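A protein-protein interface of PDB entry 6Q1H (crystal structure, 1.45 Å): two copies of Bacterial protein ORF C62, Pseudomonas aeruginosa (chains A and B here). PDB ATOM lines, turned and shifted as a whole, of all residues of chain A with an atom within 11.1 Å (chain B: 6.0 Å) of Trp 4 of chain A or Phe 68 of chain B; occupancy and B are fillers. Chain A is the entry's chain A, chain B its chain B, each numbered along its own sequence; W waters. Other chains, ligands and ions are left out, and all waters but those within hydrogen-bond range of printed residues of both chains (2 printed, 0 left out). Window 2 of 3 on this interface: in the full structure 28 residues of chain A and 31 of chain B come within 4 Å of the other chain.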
ATOM      1  N   SER A   2      23.040  -2.749   0.816  1.00  0.00           N
ATOM      2  CA  SER A   2      22.381  -2.651   2.114  1.00  0.00           C
ATOM      3  C   SER A   2      21.245  -1.629   2.086  1.00  0.00           C
ATOM      4  O   SER A   2      20.113  -1.937   2.458  1.00  0.00           O
ATOM      5  CB  SER A   2      23.386  -2.275   3.208  1.00  0.00           C
ATOM      6  OG  SER A   2      24.348  -3.298   3.401  1.00  0.00           O
ATOM      7  N   GLN A   3      21.553  -0.410   1.655  1.00  0.00           N
ATOM      8  CA  GLN A   3      20.546   0.627   1.489  1.00  0.00           C
ATOM      9  C   GLN A   3      20.094   0.647   0.036  1.00  0.00           C
ATOM     10  O   GLN A   3      20.906   0.521  -0.881  1.00  0.00           O
ATOM     11  CB  GLN A   3      21.089   1.997   1.883  1.00  0.00           C
ATOM     12  CG  GLN A   3      20.357   2.621   3.058  1.00  0.00           C
ATOM     13  CD  GLN A   3      21.294   3.347   4.002  1.00  0.00           C
ATOM     14  OE1 GLN A   3      22.315   3.895   3.587  1.00  0.00           O
ATOM     15  NE2 GLN A   3      20.957   3.342   5.286  1.00  0.00           N
ATOM     16  N   TRP A   4      18.791   0.781  -0.162  1.00  0.00           N
ATOM     17  CA  TRP A   4      18.277   0.890  -1.510  1.00  0.00           C
ATOM     18  C   TRP A   4      18.597   2.275  -2.092  1.00  0.00           C
ATOM     19  O   TRP A   4      18.481   3.296  -1.409  1.00  0.00           O
ATOM     20  CB  TRP A   4      16.768   0.736  -1.493  1.00  0.00           C
ATOM     21  CG  TRP A   4      16.195  -0.636  -1.275  1.00  0.00           C
ATOM     22  CD1 TRP A   4      15.553  -1.090  -0.155  1.00  0.00           C
ATOM     23  CD2 TRP A   4      16.157  -1.704  -2.221  1.00  0.00           C
ATOM     24  NE1 TRP A   4      15.125  -2.380  -0.357  1.00  0.00           N
ATOM     25  CE2 TRP A   4      15.490  -2.778  -1.612  1.00  0.00           C
ATOM     26  CE3 TRP A   4      16.647  -1.859  -3.519  1.00  0.00           C
ATOM     27  CZ2 TRP A   4      15.286  -3.992  -2.268  1.00  0.00           C
ATOM     28  CZ3 TRP A   4      16.437  -3.071  -4.167  1.00  0.00           C
ATOM     29  CH2 TRP A   4      15.759  -4.108  -3.542  1.00  0.00           C
ATOM     30  N   SER A   5      18.946   2.287  -3.375  1.00  0.00           N
ATOM     31  CA  SER A   5      19.255   3.505  -4.109  1.00  0.00           C
ATOM     32  C   SER A   5      18.700   3.408  -5.514  1.00  0.00           C
ATOM     33  O   SER A   5      19.091   2.517  -6.272  1.00  0.00           O
ATOM     34  CB  SER A   5      20.782   3.673  -4.190  1.00  0.00           C
ATOM     35  OG  SER A   5      21.108   4.665  -5.152  1.00  0.00           O
ATOM     36  N   LEU A   6      17.825   4.350  -5.886  1.00  0.00           N
ATOM     37  CA  LEU A   6      17.324   4.369  -7.252  1.00  0.00           C
ATOM     38  C   LEU A   6      18.454   4.627  -8.240  1.00  0.00           C
ATOM     39  O   LEU A   6      18.506   4.014  -9.306  1.00  0.00           O
ATOM     40  CB  LEU A   6      16.222   5.418  -7.394  1.00  0.00           C
ATOM     41  CG  LEU A   6      15.698   5.682  -8.800  1.00  0.00           C
ATOM     42  CD1 LEU A   6      15.187   4.436  -9.467  1.00  0.00           C
ATOM     43  CD2 LEU A   6      14.585   6.736  -8.724  1.00  0.00           C
ATOM     44  N   SER A   7      19.372   5.534  -7.902  1.00  0.00           N
ATOM     45  CA  SER A   7      20.512   5.766  -8.789  1.00  0.00           C
ATOM     46  C   SER A   7      21.284   4.480  -9.029  1.00  0.00           C
ATOM     47  O   SER A   7      21.727   4.215 -10.152  1.00  0.00           O
ATOM     48  CB  SER A   7      21.428   6.823  -8.191  1.00  0.00           C
ATOM     49  OG  SER A   7      20.786   8.075  -8.223  1.00  0.00           O
ATOM     50  N   GLN A   8      21.452   3.671  -7.984  1.00  0.00           N
ATOM     51  CA  GLN A   8      22.178   2.413  -8.147  1.00  0.00           C
ATOM     52  C   GLN A   8      21.417   1.444  -9.038  1.00  0.00           C
ATOM     53  O   GLN A   8      22.030   0.707  -9.831  1.00  0.00           O
ATOM     54  CB  GLN A   8      22.471   1.789  -6.785  1.00  0.00           C
ATOM     55  CG  GLN A   8      23.292   0.525  -6.893  1.00  0.00           C
ATOM     56  CD  GLN A   8      24.687   0.802  -7.435  1.00  0.00           C
ATOM     57  OE1 GLN A   8      25.506   1.408  -6.749  1.00  0.00           O
ATOM     58  NE2 GLN A   8      24.947   0.398  -8.670  1.00  0.00           N
ATOM     59  N   LEU A   9      20.082   1.384  -8.913  1.00  0.00           N
ATOM     60  CA  LEU A   9      19.309   0.546  -9.825  1.00  0.00           C
ATOM     61  C   LEU A   9      19.591   0.937 -11.276  1.00  0.00           C
ATOM     62  O   LEU A   9      19.851   0.083 -12.133  1.00  0.00           O
ATOM     63  CB  LEU A   9      17.812   0.662  -9.546  1.00  0.00           C
ATOM     64  CG  LEU A   9      17.242   0.307  -8.182  1.00  0.00           C
ATOM     65  CD1 LEU A   9      15.702   0.227  -8.239  1.00  0.00           C
ATOM     66  CD2 LEU A   9      17.792  -0.964  -7.698  1.00  0.00           C
ATOM     67  N   LEU A  10      19.530   2.233 -11.571  1.00  0.00           N
ATOM     68  CA  LEU A  10      19.728   2.685 -12.947  1.00  0.00           C
ATOM     69  C   LEU A  10      21.158   2.461 -13.409  1.00  0.00           C
ATOM     70  O   LEU A  10      21.391   2.121 -14.585  1.00  0.00           O
ATOM     71  CB  LEU A  10      19.352   4.155 -13.060  1.00  0.00           C
ATOM     72  CG  LEU A  10      17.911   4.486 -12.630  1.00  0.00           C
ATOM     73  CD1 LEU A  10      17.660   5.961 -12.952  1.00  0.00           C
ATOM     74  CD2 LEU A  10      16.898   3.568 -13.300  1.00  0.00           C
ATOM     75  N   SER A  11      22.129   2.637 -12.518  1.00  0.00           N
ATOM     76  CA  SER A  11      23.513   2.368 -12.887  1.00  0.00           C
ATOM     77  C   SER A  11      23.725   0.895 -13.199  1.00  0.00           C
ATOM     78  O   SER A  11      24.400   0.551 -14.174  1.00  0.00           O
ATOM     79  CB  SER A  11      24.445   2.807 -11.765  1.00  0.00           C
ATOM     80  OG  SER A  11      25.791   2.540 -12.088  1.00  0.00           O
ATOM     81  N   SER A  12      23.155   0.004 -12.380  1.00  0.00           N
ATOM     82  CA  SER A  12      23.372  -1.420 -12.585  1.00  0.00           C
ATOM     83  C   SER A  12      22.714  -1.924 -13.853  1.00  0.00           C
ATOM     84  O   SER A  12      23.260  -2.817 -14.532  1.00  0.00           O
ATOM     85  CB  SER A  12      22.845  -2.205 -11.384  1.00  0.00           C
ATOM     86  OG  SER A  12      23.665  -1.980 -10.260  1.00  0.00           O
ATOM     87  N   HIS B  60       9.717  -5.264  -4.848  1.00  0.00           N
ATOM     88  CA  HIS B  60       9.747  -3.977  -4.185  1.00  0.00           C
ATOM     89  C   HIS B  60       9.241  -2.926  -5.166  1.00  0.00           C
ATOM     90  O   HIS B  60       9.299  -3.110  -6.391  1.00  0.00           O
ATOM     91  CB  HIS B  60      11.158  -3.580  -3.755  1.00  0.00           C
ATOM     92  CG  HIS B  60      11.651  -4.294  -2.541  1.00  0.00           C
ATOM     93  ND1 HIS B  60      12.157  -5.576  -2.594  1.00  0.00           N
ATOM     94  CD2 HIS B  60      11.742  -3.892  -1.254  1.00  0.00           C
ATOM     95  CE1 HIS B  60      12.525  -5.935  -1.376  1.00  0.00           C
ATOM     96  NE2 HIS B  60      12.294  -4.932  -0.548  1.00  0.00           N
ATOM     97  N   VAL B  61       8.743  -1.829  -4.616  1.00  0.00           N
ATOM     98  CA  VAL B  61       8.242  -0.690  -5.391  1.00  0.00           C
ATOM     99  C   VAL B  61       9.148   0.509  -5.120  1.00  0.00           C
ATOM    100  O   VAL B  61       9.568   0.746  -3.985  1.00  0.00           O
ATOM    101  CB  VAL B  61       6.784  -0.363  -5.017  1.00  0.00           C
ATOM    102  CG1 VAL B  61       6.216   0.661  -5.971  1.00  0.00           C
ATOM    103  CG2 VAL B  61       5.920  -1.638  -5.055  1.00  0.00           C
ATOM    104  N   VAL B  62       9.449   1.273  -6.177  1.00  0.00           N
ATOM    105  CA  VAL B  62      10.258   2.490  -6.056  1.00  0.00           C
ATOM    106  C   VAL B  62       9.509   3.623  -6.740  1.00  0.00           C
ATOM    107  O   VAL B  62       8.700   3.378  -7.652  1.00  0.00           O
ATOM    108  CB  VAL B  62      11.660   2.275  -6.683  1.00  0.00           C
ATOM    109  CG1 VAL B  62      11.571   2.121  -8.167  1.00  0.00           C
ATOM    110  CG2 VAL B  62      12.620   3.387  -6.331  1.00  0.00           C
ATOM    111  N   ASP B  63       9.798   4.855  -6.318  1.00  0.00           N
ATOM    112  CA  ASP B  63       9.232   6.024  -6.994  1.00  0.00           C
ATOM    113  C   ASP B  63      10.319   6.952  -7.528  1.00  0.00           C
ATOM    114  O   ASP B  63      11.512   6.752  -7.311  1.00  0.00           O
ATOM    115  CB  ASP B  63       8.193   6.766  -6.118  1.00  0.00           C
ATOM    116  CG  ASP B  63       8.803   7.532  -4.950  1.00  0.00           C
ATOM    117  OD1 ASP B  63      10.030   7.728  -4.884  1.00  0.00           O
ATOM    118  OD2 ASP B  63       8.006   8.000  -4.088  1.00  0.00           O
ATOM    119  N   GLY B  66      13.024   8.512  -5.451  1.00  0.00           N
ATOM    120  CA  GLY B  66      14.048   7.657  -4.874  1.00  0.00           C
ATOM    121  C   GLY B  66      13.633   6.895  -3.650  1.00  0.00           C
ATOM    122  O   GLY B  66      14.484   6.291  -2.989  1.00  0.00           O
ATOM    123  N   ASN B  67      12.350   6.908  -3.299  1.00  0.00           N
ATOM    124  CA  ASN B  67      11.881   6.169  -2.136  1.00  0.00           C
ATOM    125  C   ASN B  67      11.360   4.791  -2.503  1.00  0.00           C
ATOM    126  O   ASN B  67      10.864   4.552  -3.601  1.00  0.00           O
ATOM    127  CB  ASN B  67      10.819   7.007  -1.415  1.00  0.00           C
ATOM    128  CG  ASN B  67      11.416   8.256  -0.816  1.00  0.00           C
ATOM    129  OD1 ASN B  67      12.519   8.228  -0.253  1.00  0.00           O
ATOM    130  ND2 ASN B  67      10.733   9.376  -0.978  1.00  0.00           N
ATOM    131  N   PHE B  68      11.518   3.863  -1.552  1.00  0.00           N
ATOM    132  CA  PHE B  68      11.182   2.466  -1.749  1.00  0.00           C
ATOM    133  C   PHE B  68      10.127   2.002  -0.753  1.00  0.00           C
ATOM    134  O   PHE B  68      10.110   2.443   0.412  1.00  0.00           O
ATOM    135  CB  PHE B  68      12.443   1.573  -1.570  1.00  0.00           C
ATOM    136  CG  PHE B  68      13.447   1.691  -2.679  1.00  0.00           C
ATOM    137  CD1 PHE B  68      14.242   2.816  -2.787  1.00  0.00           C
ATOM    138  CD2 PHE B  68      13.589   0.674  -3.603  1.00  0.00           C
ATOM    139  CE1 PHE B  68      15.160   2.939  -3.803  1.00  0.00           C
ATOM    140  CE2 PHE B  68      14.524   0.790  -4.644  1.00  0.00           C
ATOM    141  CZ  PHE B  68      15.317   1.919  -4.719  1.00  0.00           C
ATOM    142  N   SER B  69       9.268   1.104  -1.220  1.00  0.00           N
ATOM    143  CA  SER B  69       8.355   0.407  -0.339  1.00  0.00           C
ATOM    144  C   SER B  69       9.095  -0.687   0.444  1.00  0.00           C
ATOM    145  O   SER B  69      10.281  -0.948   0.252  1.00  0.00           O
ATOM    146  CB  SER B  69       7.236  -0.268  -1.139  1.00  0.00           C
ATOM    147  OG  SER B  69       7.712  -1.385  -1.878  1.00  0.00           O
ATOM    148  N   GLN B  70       8.365  -1.320   1.349  1.00  0.00           N
ATOM    149  CA  GLN B  70       8.817  -2.584   1.909  1.00  0.00           C
ATOM    150  C   GLN B  70       8.715  -3.671   0.834  1.00  0.00           C
ATOM    151  O   GLN B  70       8.121  -3.487  -0.237  1.00  0.00           O
ATOM    152  CB  GLN B  70       7.956  -2.952   3.115  1.00  0.00           C
ATOM    153  CG  GLN B  70       8.116  -2.044   4.322  1.00  0.00           C
ATOM    154  CD  GLN B  70       7.246  -2.504   5.487  1.00  0.00           C
ATOM    155  OE1 GLN B  70       6.308  -1.813   5.873  1.00  0.00           O
ATOM    156  NE2 GLN B  70       7.548  -3.677   6.037  1.00  0.00           N
ATOM    157  N   ILE B  93      12.160  -4.860  -9.084  1.00  0.00           N
ATOM    158  CA  ILE B  93      11.714  -3.578  -8.547  1.00  0.00           C
ATOM    159  C   ILE B  93      10.858  -2.908  -9.618  1.00  0.00           C
ATOM    160  O   ILE B  93      11.316  -2.713 -10.753  1.00  0.00           O
ATOM    161  CB  ILE B  93      12.882  -2.678  -8.131  1.00  0.00           C
ATOM    162  CG1 ILE B  93      13.721  -3.353  -7.046  1.00  0.00           C
ATOM    163  CG2 ILE B  93      12.333  -1.338  -7.602  1.00  0.00           C
ATOM    164  CD1 ILE B  93      14.890  -4.099  -7.567  1.00  0.00           C
ATOM    165  N   SER B 123       3.351   1.677   2.966  1.00  0.00           N
ATOM    166  CA  SER B 123       4.691   1.920   2.423  1.00  0.00           C
ATOM    167  C   SER B 123       4.662   2.089   0.909  1.00  0.00           C
ATOM    168  O   SER B 123       5.587   2.693   0.353  1.00  0.00           O
ATOM    169  CB  SER B 123       5.658   0.796   2.795  1.00  0.00           C
ATOM    170  OG  SER B 123       5.481  -0.339   1.983  1.00  0.00           O
ATOM    171  N   LEU B 127       4.252   6.469  -1.653  1.00  0.00           N
ATOM    172  CA  LEU B 127       5.130   6.782  -2.769  1.00  0.00           C
ATOM    173  C   LEU B 127       4.457   7.744  -3.739  1.00  0.00           C
ATOM    174  O   LEU B 127       3.233   7.792  -3.859  1.00  0.00           O
ATOM    175  CB  LEU B 127       5.513   5.508  -3.513  1.00  0.00           C
ATOM    176  CG  LEU B 127       6.285   4.487  -2.675  1.00  0.00           C
ATOM    177  CD1 LEU B 127       6.534   3.234  -3.504  1.00  0.00           C
ATOM    178  CD2 LEU B 127       7.596   5.065  -2.147  1.00  0.00           C
HETATM  179  O   HOH W   1      13.308  -3.700   1.872  1.00  0.00           O
HETATM  180  O   HOH W   2      17.037   6.245  -3.815  1.00  0.00           O
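N of Ser 7 of chain A lies close to OG of Ser 5 of chain A (3.4 Å).
N of Gln 8 of chain A sits at hydrogen-bond distance from OG of Ser 5 of chain A (3.0 Å).
The side-chain carboxylate of Asp 63 of chain B is in hydrogen-bond range of the backbone NH of Gly 66 of chain B (3.1 Å).
The side-chain carboxylate (OD1) of Asp 63 of chain B lies within hydrogen-bond range of the backbone NH (N) of Asn 67 of chain B.
Among the printed residues, pairs that only touch across the chains: Leu 6 of chain A with Asp 63 of chain B, Trp 4 of chain A with His 60 of chain B, Trp 4 of chain A with Phe 68 of chain B, Leu 6 of chain A with Phe 68 of chain B, Leu 9 of chain A with Ile 93 of chain B, Ser 5 of chain A with Phe 68 of chain B, Leu 9 of chain A with Phe 68 of chain B, Trp 4 of chain A with Ile 93 of chain B and Leu 6 of chain A with Gly 66 of chain B.
Of chain B, only His 60 (3.5 Å), Phe 68 (3.5 Å) and Ile 93 (3.9 Å) come within 4 Å of Trp 4 of chain A.
Of the printed residues of chain B, Ser 5 of chain A touches Phe 68 (3.8 Å).
Printed residues of chain B within 4 Å of Leu 6 of chain A: Asp 63 (3.4 Å), Gly 66 (3.99 Å) and Phe 68 (3.7 Å).
Printed residues of chain B within 4 Å of Leu 9 of chain A: Phe 68 (3.8 Å) and Ile 93 (3.8 Å).
His 60 of chain B touches one residue of chain A.
No residue of chain A comes within 4 Å of Val 62 of chain B.
Printed residues of chain A within 4 Å of Asp 63 of chain B: Leu 6 (3.4 Å).
Of the printed residues of chain A, Gly 66 of chain B touches Leu 6 (3.99 Å).
No residue of chain A comes within 4 Å of Asn 67 of chain B.
Phe 68 of chain B touches just these residues of chain A: Trp 4 (3.5 Å), Ser 5 (3.8 Å), Leu 6 (3.7 Å) and Leu 9 (3.8 Å).
Gln 70 of chain B touches none of the printed residues of chain A.
The nearest residue of chain B that does not touch Trp 4 of chain A is Ser 69 of chain B (5.1 Å).
The nearest printed residue of chain A that does not touch Phe 68 of chain B is Ser 7 of chain A (6.3 Å).
The nearest printed residue of chain B that does not touch Ser 5 of chain A is Gly 66 of chain B (5.6 Å).
Of the 11 printed residues of chain A, 4 touch a printed residue of chain B.
Along chain A the printed residues that touch a printed residue of chain B span positions 4 to 9.
Of the 12 printed residues of chain B, 5 touch a printed residue of chain A.
Hydrophobic or aromatic side chains of chain B that line the printed part of chain A: His 60, Phe 68 and Ile 93.
Among the printed residues, no Asp or Glu carboxylate lies within 4 Å of a Lys or Arg side-chain nitrogen of the other chain.
No position is printed for both chains.
Of the 9 pairs that touch across the chains among the printed residues, none has its exchanged pair printed and touching as well.
Water W2 lies within hydrogen-bond range of O of Gly 66 of chain B (2.7 Å) and N of Leu 6 of chain A (2.9 Å).
Water W1 lies within hydrogen-bond range of NE2 of His 60 of chain B (2.9 Å) and NE1 of Trp 4 of chain A (3.2 Å).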
